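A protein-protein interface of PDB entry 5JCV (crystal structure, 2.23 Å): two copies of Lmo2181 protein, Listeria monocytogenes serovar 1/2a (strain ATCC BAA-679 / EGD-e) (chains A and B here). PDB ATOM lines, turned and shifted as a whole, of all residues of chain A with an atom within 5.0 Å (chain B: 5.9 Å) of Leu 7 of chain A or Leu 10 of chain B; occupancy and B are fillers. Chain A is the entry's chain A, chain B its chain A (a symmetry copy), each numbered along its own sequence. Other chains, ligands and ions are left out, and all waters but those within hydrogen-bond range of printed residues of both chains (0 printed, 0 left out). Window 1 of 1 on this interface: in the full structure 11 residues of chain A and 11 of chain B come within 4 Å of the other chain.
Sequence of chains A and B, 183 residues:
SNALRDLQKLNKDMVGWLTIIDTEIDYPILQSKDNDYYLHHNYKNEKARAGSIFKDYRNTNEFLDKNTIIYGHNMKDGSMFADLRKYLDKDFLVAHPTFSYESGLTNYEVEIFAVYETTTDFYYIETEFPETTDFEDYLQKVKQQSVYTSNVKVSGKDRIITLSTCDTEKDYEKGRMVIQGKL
NE2 of Gln 8 of chain A sits close to NE1 of Trp 17 of chain B (3.4 Å). The side-chain amide nitrogen (ND2) of Asn 11 of chain A lies close to the side-chain sulfur (SD) of Met 14 of chain B, 3.6 Å away.
Leu 7 of chain A touches Leu 10 of chain B, and with the chains exchanged Leu 10 of chain A touches Leu 7 of chain B. Positions printed for both chains: 5, 6, 7, 8, 9, 10 and 11. Of the 8 pairs that touch across the chains among the printed residues, 2 have their exchanged pair printed and touching as well.
Trp 17 of chain B touches Leu 4 of chain A (CH2 to O, 3.8 Å). Leu 7 of chain A touches Leu 10 of chain B (CD1 to CD2, 3.9 Å). Trp 17 of chain B touches Leu 7 of chain A. Pro 28 of chain B touches Leu 7 of chain A (CG to CD2, 3.9 Å). CD2 of Leu 7 of chain A touches CE1 of Tyr 43 of chain B (3.9 Å). CD2 of Leu 10 of chain A touches CD1 of Leu 7 of chain B (3.9 Å).
Of the 9 printed residues of chain A, 5 touch a printed residue of chain B. Of the 16 printed residues of chain B, 6 touch a printed residue of chain A. Hydrophobic or aromatic side chains of chain B within 4 Å of the printed part of chain A: Leu 7, Leu 10, Met 14, Trp 17, Pro 28 and Tyr 43. Among the printed residues, 8 pairs touch across the chains. Among the printed residues, no Asp or Glu carboxylate lies within 4 Å of a Lys or Arg side-chain nitrogen of the other chain.
Of the printed residues of chain B, Leu 7 of chain A touches Leu 10 (3.9 Å), Trp 17 (3.998 Å), Pro 28 (3.9 Å) and Tyr 43 (3.9 Å). Of the printed residues of chain A, Leu 10 of chain B touches Leu 7. Printed residues of chain B within 4 Å of Asn 11 of chain A: Met 14. Of the printed residues of chain A, Pro 28 of chain B touches Leu 7. Of the printed residues of chain B, Leu 10 of chain A touches Leu 7 (3.9 Å). Of the printed residues of chain A, Trp 17 of chain B touches Leu 4, Leu 7 and Gln 8. Printed residues of chain B within 4 Å of Gln 8 of chain A: Trp 17 (3.4 Å). Asp 13 of chain B touches none of the printed residues of chain A. Asp 6 of chain A touches none of the printed residues of chain B. The nearest printed residue of chain B that does not touch Leu 7 of chain A is Met 14 of chain B (4.4 Å).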
ATOM      1  N   ALA A   3     -20.449 -39.130 -13.339  1.00  0.00           N
ATOM      2  CA  ALA A   3     -21.606 -38.527 -12.602  1.00  0.00           C
ATOM      3  C   ALA A   3     -21.294 -37.146 -12.004  1.00  0.00           C
ATOM      4  O   ALA A   3     -22.185 -36.379 -11.655  1.00  0.00           O
ATOM      5  CB  ALA A   3     -22.058 -39.474 -11.502  1.00  0.00           C
ATOM      6  N   LEU A   4     -20.016 -36.844 -11.855  1.00  0.00           N
ATOM      7  CA  LEU A   4     -19.597 -35.518 -11.446  1.00  0.00           C
ATOM      8  C   LEU A   4     -19.466 -34.591 -12.657  1.00  0.00           C
ATOM      9  O   LEU A   4     -19.519 -33.373 -12.519  1.00  0.00           O
ATOM     10  CB  LEU A   4     -18.296 -35.622 -10.664  1.00  0.00           C
ATOM     11  CG  LEU A   4     -17.661 -34.308 -10.241  1.00  0.00           C
ATOM     12  CD1 LEU A   4     -17.220 -34.374  -8.783  1.00  0.00           C
ATOM     13  CD2 LEU A   4     -16.512 -34.009 -11.205  1.00  0.00           C
ATOM     14  N   ARG A   5     -19.303 -35.177 -13.839  1.00  0.00           N
ATOM     15  CA  ARG A   5     -19.411 -34.443 -15.098  1.00  0.00           C
ATOM     16  C   ARG A   5     -20.831 -33.865 -15.244  1.00  0.00           C
ATOM     17  O   ARG A   5     -21.029 -32.719 -15.659  1.00  0.00           O
ATOM     18  CB  ARG A   5     -19.066 -35.372 -16.282  1.00  0.00           C
ATOM     19  CG  ARG A   5     -20.123 -36.444 -16.544  1.00  0.00           C
ATOM     20  CD  ARG A   5     -19.583 -37.766 -17.062  1.00  0.00           C
ATOM     21  NE  ARG A   5     -20.299 -38.872 -16.421  1.00  0.00           N
ATOM     22  CZ  ARG A   5     -20.163 -40.151 -16.752  1.00  0.00           C
ATOM     23  NH1 ARG A   5     -19.351 -40.515 -17.745  1.00  0.00           N
ATOM     24  NH2 ARG A   5     -20.853 -41.072 -16.094  1.00  0.00           N
ATOM     25  N   ASP A   6     -21.825 -34.661 -14.873  1.00  0.00           N
ATOM     26  CA  ASP A   6     -23.209 -34.220 -14.948  1.00  0.00           C
ATOM     27  C   ASP A   6     -23.444 -33.128 -13.893  1.00  0.00           C
ATOM     28  O   ASP A   6     -24.122 -32.150 -14.149  1.00  0.00           O
ATOM     29  CB  ASP A   6     -24.171 -35.421 -14.786  1.00  0.00           C
ATOM     30  CG  ASP A   6     -24.083 -36.437 -15.971  1.00  0.00           C
ATOM     31  OD1 ASP A   6     -23.716 -36.033 -17.099  1.00  0.00           O
ATOM     32  OD2 ASP A   6     -24.383 -37.643 -15.772  1.00  0.00           O
ATOM     33  N   LEU A   7     -22.832 -33.259 -12.720  1.00  0.00           N
ATOM     34  CA  LEU A   7     -22.982 -32.225 -11.682  1.00  0.00           C
ATOM     35  C   LEU A   7     -22.420 -30.858 -12.111  1.00  0.00           C
ATOM     36  O   LEU A   7     -23.027 -29.836 -11.851  1.00  0.00           O
ATOM     37  CB  LEU A   7     -22.313 -32.674 -10.387  1.00  0.00           C
ATOM     38  CG  LEU A   7     -22.609 -31.772  -9.189  1.00  0.00           C
ATOM     39  CD1 LEU A   7     -24.094 -31.851  -8.879  1.00  0.00           C
ATOM     40  CD2 LEU A   7     -21.778 -32.150  -7.970  1.00  0.00           C
ATOM     41  N   GLN A   8     -21.258 -30.851 -12.758  1.00  0.00           N
ATOM     42  CA  GLN A   8     -20.684 -29.615 -13.300  1.00  0.00           C
ATOM     43  C   GLN A   8     -21.611 -28.958 -14.336  1.00  0.00           C
ATOM     44  O   GLN A   8     -21.796 -27.748 -14.300  1.00  0.00           O
ATOM     45  CB  GLN A   8     -19.297 -29.877 -13.901  1.00  0.00           C
ATOM     46  CG  GLN A   8     -18.661 -28.630 -14.507  1.00  0.00           C
ATOM     47  CD  GLN A   8     -17.170 -28.741 -14.789  1.00  0.00           C
ATOM     48  OE1 GLN A   8     -16.615 -29.812 -15.137  1.00  0.00           O
ATOM     49  NE2 GLN A   8     -16.499 -27.604 -14.634  1.00  0.00           N
ATOM     50  N   LYS A   9     -22.167 -29.769 -15.245  1.00  0.00           N
ATOM     51  CA  LYS A   9     -23.203 -29.355 -16.204  1.00  0.00           C
ATOM     52  C   LYS A   9     -24.362 -28.669 -15.508  1.00  0.00           C
ATOM     53  O   LYS A   9     -24.741 -27.557 -15.849  1.00  0.00           O
ATOM     54  CB  LYS A   9     -23.799 -30.570 -16.954  1.00  0.00           C
ATOM     55  CG  LYS A   9     -23.183 -30.920 -18.304  1.00  0.00           C
ATOM     56  CD  LYS A   9     -24.069 -31.935 -19.041  1.00  0.00           C
ATOM     57  CE  LYS A   9     -23.360 -32.616 -20.212  1.00  0.00           C
ATOM     58  NZ  LYS A   9     -22.357 -33.637 -19.771  1.00  0.00           N
ATOM     59  N   LEU A  10     -24.929 -29.352 -14.522  1.00  0.00           N
ATOM     60  CA  LEU A  10     -26.049 -28.808 -13.758  1.00  0.00           C
ATOM     61  C   LEU A  10     -25.744 -27.454 -13.124  1.00  0.00           C
ATOM     62  O   LEU A  10     -26.601 -26.602 -13.057  1.00  0.00           O
ATOM     63  CB  LEU A  10     -26.466 -29.818 -12.685  1.00  0.00           C
ATOM     64  CG  LEU A  10     -27.575 -29.411 -11.706  1.00  0.00           C
ATOM     65  CD1 LEU A  10     -28.846 -29.126 -12.492  1.00  0.00           C
ATOM     66  CD2 LEU A  10     -27.816 -30.482 -10.641  1.00  0.00           C
ATOM     67  N   ASN A  11     -24.511 -27.261 -12.657  1.00  0.00           N
ATOM     68  CA  ASN A  11     -24.109 -26.018 -11.988  1.00  0.00           C
ATOM     69  C   ASN A  11     -23.994 -24.826 -12.922  1.00  0.00           C
ATOM     70  O   ASN A  11     -24.134 -23.701 -12.508  1.00  0.00           O
ATOM     71  CB  ASN A  11     -22.770 -26.214 -11.279  1.00  0.00           C
ATOM     72  CG  ASN A  11     -22.291 -24.962 -10.604  1.00  0.00           C
ATOM     73  OD1 ASN A  11     -21.330 -24.338 -11.045  1.00  0.00           O
ATOM     74  ND2 ASN A  11     -22.951 -24.586  -9.486  1.00  0.00           N
ATOM     75  N   ARG B   5     -36.459 -31.635  -3.140  1.00  0.00           N
ATOM     76  CA  ARG B   5     -36.079 -30.925  -1.922  1.00  0.00           C
ATOM     77  C   ARG B   5     -34.543 -30.898  -1.794  1.00  0.00           C
ATOM     78  O   ARG B   5     -33.937 -29.882  -1.439  1.00  0.00           O
ATOM     79  CB  ARG B   5     -36.726 -31.599  -0.694  1.00  0.00           C
ATOM     80  CG  ARG B   5     -36.130 -32.967  -0.364  1.00  0.00           C
ATOM     81  CD  ARG B   5     -37.109 -33.971   0.219  1.00  0.00           C
ATOM     82  NE  ARG B   5     -36.853 -35.294  -0.352  1.00  0.00           N
ATOM     83  CZ  ARG B   5     -37.442 -36.416   0.045  1.00  0.00           C
ATOM     84  NH1 ARG B   5     -38.321 -36.405   1.047  1.00  0.00           N
ATOM     85  NH2 ARG B   5     -37.143 -37.559  -0.556  1.00  0.00           N
ATOM     86  N   ASP B   6     -33.913 -32.020  -2.111  1.00  0.00           N
ATOM     87  CA  ASP B   6     -32.463 -32.110  -2.046  1.00  0.00           C
ATOM     88  C   ASP B   6     -31.855 -31.238  -3.155  1.00  0.00           C
ATOM     89  O   ASP B   6     -30.865 -30.563  -2.946  1.00  0.00           O
ATOM     90  CB  ASP B   6     -32.005 -33.587  -2.133  1.00  0.00           C
ATOM     91  CG  ASP B   6     -32.448 -34.435  -0.896  1.00  0.00           C
ATOM     92  OD1 ASP B   6     -32.629 -33.865   0.206  1.00  0.00           O
ATOM     93  OD2 ASP B   6     -32.608 -35.676  -1.026  1.00  0.00           O
ATOM     94  N   LEU B   7     -32.486 -31.199  -4.326  1.00  0.00           N
ATOM     95  CA  LEU B   7     -31.979 -30.350  -5.417  1.00  0.00           C
ATOM     96  C   LEU B   7     -31.999 -28.851  -5.068  1.00  0.00           C
ATOM     97  O   LEU B   7     -31.065 -28.137  -5.376  1.00  0.00           O
ATOM     98  CB  LEU B   7     -32.779 -30.592  -6.692  1.00  0.00           C
ATOM     99  CG  LEU B   7     -32.187 -29.927  -7.934  1.00  0.00           C
ATOM    100  CD1 LEU B   7     -30.836 -30.558  -8.225  1.00  0.00           C
ATOM    101  CD2 LEU B   7     -33.110 -30.041  -9.139  1.00  0.00           C
ATOM    102  N   GLN B   8     -33.073 -28.385  -4.434  1.00  0.00           N
ATOM    103  CA  GLN B   8     -33.151 -26.998  -3.965  1.00  0.00           C
ATOM    104  C   GLN B   8     -32.038 -26.670  -2.957  1.00  0.00           C
ATOM    105  O   GLN B   8     -31.424 -25.614  -3.056  1.00  0.00           O
ATOM    106  CB  GLN B   8     -34.531 -26.704  -3.365  1.00  0.00           C
ATOM    107  CG  GLN B   8     -34.662 -25.280  -2.834  1.00  0.00           C
ATOM    108  CD  GLN B   8     -36.089 -24.824  -2.560  1.00  0.00           C
ATOM    109  OE1 GLN B   8     -36.993 -25.599  -2.161  1.00  0.00           O
ATOM    110  NE2 GLN B   8     -36.301 -23.530  -2.784  1.00  0.00           N
ATOM    111  N   LYS B   9     -31.806 -27.578  -2.000  1.00  0.00           N
ATOM    112  CA  LYS B   9     -30.681 -27.519  -1.053  1.00  0.00           C
ATOM    113  C   LYS B   9     -29.359 -27.340  -1.774  1.00  0.00           C
ATOM    114  O   LYS B   9     -28.597 -26.427  -1.490  1.00  0.00           O
ATOM    115  CB  LYS B   9     -30.560 -28.825  -0.234  1.00  0.00           C
ATOM    116  CG  LYS B   9     -31.248 -28.853   1.128  1.00  0.00           C
ATOM    117  CD  LYS B   9     -30.786 -30.080   1.927  1.00  0.00           C
ATOM    118  CE  LYS B   9     -31.682 -30.391   3.127  1.00  0.00           C
ATOM    119  NZ  LYS B   9     -32.994 -30.997   2.731  1.00  0.00           N
ATOM    120  N   LEU B  10     -29.089 -28.236  -2.716  1.00  0.00           N
ATOM    121  CA  LEU B  10     -27.857 -28.179  -3.496  1.00  0.00           C
ATOM    122  C   LEU B  10     -27.652 -26.844  -4.206  1.00  0.00           C
ATOM    123  O   LEU B  10     -26.545 -26.368  -4.310  1.00  0.00           O
ATOM    124  CB  LEU B  10     -27.847 -29.327  -4.509  1.00  0.00           C
ATOM    125  CG  LEU B  10     -26.676 -29.408  -5.498  1.00  0.00           C
ATOM    126  CD1 LEU B  10     -25.381 -29.564  -4.715  1.00  0.00           C
ATOM    127  CD2 LEU B  10     -26.854 -30.548  -6.499  1.00  0.00           C
ATOM    128  N   ASN B  11     -28.736 -26.240  -4.695  1.00  0.00           N
ATOM    129  CA  ASN B  11     -28.663 -24.975  -5.435  1.00  0.00           C
ATOM    130  C   ASN B  11     -28.327 -23.774  -4.566  1.00  0.00           C
ATOM    131  O   ASN B  11     -27.789 -22.801  -5.039  1.00  0.00           O
ATOM    132  CB  ASN B  11     -29.988 -24.706  -6.145  1.00  0.00           C
ATOM    133  CG  ASN B  11     -29.985 -23.403  -6.892  1.00  0.00           C
ATOM    134  OD1 ASN B  11     -30.649 -22.451  -6.495  1.00  0.00           O
ATOM    135  ND2 ASN B  11     -29.245 -23.356  -8.022  1.00  0.00           N
ATOM    136  N   LYS B  12     -28.691 -23.807  -3.311  1.00  0.00           N
ATOM    137  CA  LYS B  12     -28.204 -22.793  -2.375  1.00  0.00           C
ATOM    138  C   LYS B  12     -26.752 -23.075  -1.864  1.00  0.00           C
ATOM    139  O   LYS B  12     -25.953 -22.157  -1.668  1.00  0.00           O
ATOM    140  CB  LYS B  12     -29.144 -22.751  -1.177  1.00  0.00           C
ATOM    141  CG  LYS B  12     -28.866 -21.626  -0.184  1.00  0.00           C
ATOM    142  CD  LYS B  12     -29.870 -21.630   0.956  1.00  0.00           C
ATOM    143  CE  LYS B  12     -29.621 -22.790   1.901  1.00  0.00           C
ATOM    144  NZ  LYS B  12     -30.656 -22.819   2.982  1.00  0.00           N
ATOM    145  N   ASP B  13     -26.438 -24.345  -1.635  1.00  0.00           N
ATOM    146  CA  ASP B  13     -25.175 -24.750  -1.011  1.00  0.00           C
ATOM    147  C   ASP B  13     -23.994 -24.625  -1.967  1.00  0.00           C
ATOM    148  O   ASP B  13     -22.920 -24.207  -1.541  1.00  0.00           O
ATOM    149  CB  ASP B  13     -25.269 -26.206  -0.551  1.00  0.00           C
ATOM    150  CG  ASP B  13     -26.285 -26.411   0.549  1.00  0.00           C
ATOM    151  OD1 ASP B  13     -26.723 -25.438   1.184  1.00  0.00           O
ATOM    152  OD2 ASP B  13     -26.647 -27.568   0.798  1.00  0.00           O
ATOM    153  N   MET B  14     -24.187 -24.980  -3.251  1.00  0.00           N
ATOM    154  CA  MET B  14     -23.074 -25.000  -4.236  1.00  0.00           C
ATOM    155  C   MET B  14     -22.940 -23.637  -4.809  1.00  0.00           C
ATOM    156  O   MET B  14     -23.847 -23.149  -5.411  1.00  0.00           O
ATOM    157  CB  MET B  14     -23.244 -26.104  -5.284  1.00  0.00           C
ATOM    158  CG  MET B  14     -22.473 -25.953  -6.606  1.00  0.00           C
ATOM    159  SD  MET B  14     -22.704 -27.661  -7.586  1.00  0.00           S
ATOM    160  CE  MET B  14     -24.594 -27.410  -8.155  1.00  0.00           C
ATOM    161  N   VAL B  15     -21.784 -23.018  -4.611  1.00  0.00           N
ATOM    162  CA  VAL B  15     -21.534 -21.578  -4.824  1.00  0.00           C
ATOM    163  C   VAL B  15     -20.482 -21.371  -5.929  1.00  0.00           C
ATOM    164  O   VAL B  15     -20.020 -20.246  -6.190  1.00  0.00           O
ATOM    165  CB  VAL B  15     -21.073 -21.010  -3.453  1.00  0.00           C
ATOM    166  CG1 VAL B  15     -20.022 -19.907  -3.539  1.00  0.00           C
ATOM    167  CG2 VAL B  15     -22.291 -20.553  -2.645  1.00  0.00           C
ATOM    168  N   TRP B  17     -17.328 -23.667  -8.706  1.00  0.00           N
ATOM    169  CA  TRP B  17     -16.645 -24.855  -9.236  1.00  0.00           C
ATOM    170  C   TRP B  17     -15.147 -24.564  -9.293  1.00  0.00           C
ATOM    171  O   TRP B  17     -14.735 -23.413  -9.498  1.00  0.00           O
ATOM    172  CB  TRP B  17     -17.142 -25.259 -10.636  1.00  0.00           C
ATOM    173  CG  TRP B  17     -16.778 -26.652 -10.914  1.00  0.00           C
ATOM    174  CD1 TRP B  17     -15.605 -27.098 -11.385  1.00  0.00           C
ATOM    175  CD2 TRP B  17     -17.579 -27.810 -10.666  1.00  0.00           C
ATOM    176  NE1 TRP B  17     -15.617 -28.461 -11.480  1.00  0.00           N
ATOM    177  CE2 TRP B  17     -16.815 -28.919 -11.006  1.00  0.00           C
ATOM    178  CE3 TRP B  17     -18.882 -28.005 -10.189  1.00  0.00           C
ATOM    179  CZ2 TRP B  17     -17.302 -30.221 -10.904  1.00  0.00           C
ATOM    180  CZ3 TRP B  17     -19.360 -29.301 -10.063  1.00  0.00           C
ATOM    181  CH2 TRP B  17     -18.573 -30.392 -10.422  1.00  0.00           C
ATOM    182  N   PRO B  28     -17.220 -29.279  -7.129  1.00  0.00           N
ATOM    183  CA  PRO B  28     -18.092 -28.215  -6.733  1.00  0.00           C
ATOM    184  C   PRO B  28     -17.544 -27.555  -5.480  1.00  0.00           C
ATOM    185  O   PRO B  28     -16.897 -28.219  -4.643  1.00  0.00           O
ATOM    186  CB  PRO B  28     -19.406 -28.933  -6.451  1.00  0.00           C
ATOM    187  CG  PRO B  28     -18.964 -30.280  -5.971  1.00  0.00           C
ATOM    188  CD  PRO B  28     -17.860 -30.589  -6.937  1.00  0.00           C
ATOM    189  N   LEU B  30     -18.670 -25.696  -2.220  1.00  0.00           N
ATOM    190  CA  LEU B  30     -19.814 -25.518  -1.346  1.00  0.00           C
ATOM    191  C   LEU B  30     -19.559 -24.395  -0.358  1.00  0.00           C
ATOM    192  O   LEU B  30     -18.494 -23.825  -0.383  1.00  0.00           O
ATOM    193  CB  LEU B  30     -20.204 -26.860  -0.693  1.00  0.00           C
ATOM    194  CG  LEU B  30     -20.951 -27.633  -1.815  1.00  0.00           C
ATOM    195  CD1 LEU B  30     -20.028 -28.548  -2.637  1.00  0.00           C
ATOM    196  CD2 LEU B  30     -22.166 -28.396  -1.306  1.00  0.00           C
ATOM    197  N   TYR B  43     -21.451 -33.057  -0.859  1.00  0.00           N
ATOM    198  CA  TYR B  43     -22.216 -32.023  -1.552  1.00  0.00           C
ATOM    199  C   TYR B  43     -23.747 -32.232  -1.463  1.00  0.00           C
ATOM    200  O   TYR B  43     -24.515 -31.320  -1.769  1.00  0.00           O
ATOM    201  CB  TYR B  43     -21.755 -31.872  -3.015  1.00  0.00           C
ATOM    202  CG  TYR B  43     -22.109 -33.029  -3.927  1.00  0.00           C
ATOM    203  CD1 TYR B  43     -23.387 -33.154  -4.472  1.00  0.00           C
ATOM    204  CD2 TYR B  43     -21.157 -33.996  -4.251  1.00  0.00           C
ATOM    205  CE1 TYR B  43     -23.711 -34.227  -5.286  1.00  0.00           C
ATOM    206  CE2 TYR B  43     -21.469 -35.054  -5.074  1.00  0.00           C
ATOM    207  CZ  TYR B  43     -22.748 -35.171  -5.579  1.00  0.00           C
ATOM    208  OH  TYR B  43     -23.049 -36.225  -6.398  1.00  0.00           O
ATOM    209  N   LYS B  44     -24.163 -33.433  -1.066  1.00  0.00           N
ATOM    210  CA  LYS B  44     -25.572 -33.765  -0.860  1.00  0.00           C
ATOM    211  C   LYS B  44     -25.991 -33.556   0.592  1.00  0.00           C
ATOM    212  O   LYS B  44     -27.098 -33.926   0.984  1.00  0.00           O
ATOM    213  CB  LYS B  44     -25.817 -35.232  -1.234  1.00  0.00           C
ATOM    214  CG  LYS B  44     -25.693 -35.549  -2.725  1.00  0.00           C
ATOM    215  CD  LYS B  44     -25.993 -37.016  -2.985  1.00  0.00           C
ATOM    216  CE  LYS B  44     -25.806 -37.375  -4.446  1.00  0.00           C
ATOM    217  NZ  LYS B  44     -25.959 -38.839  -4.684  1.00  0.00           N
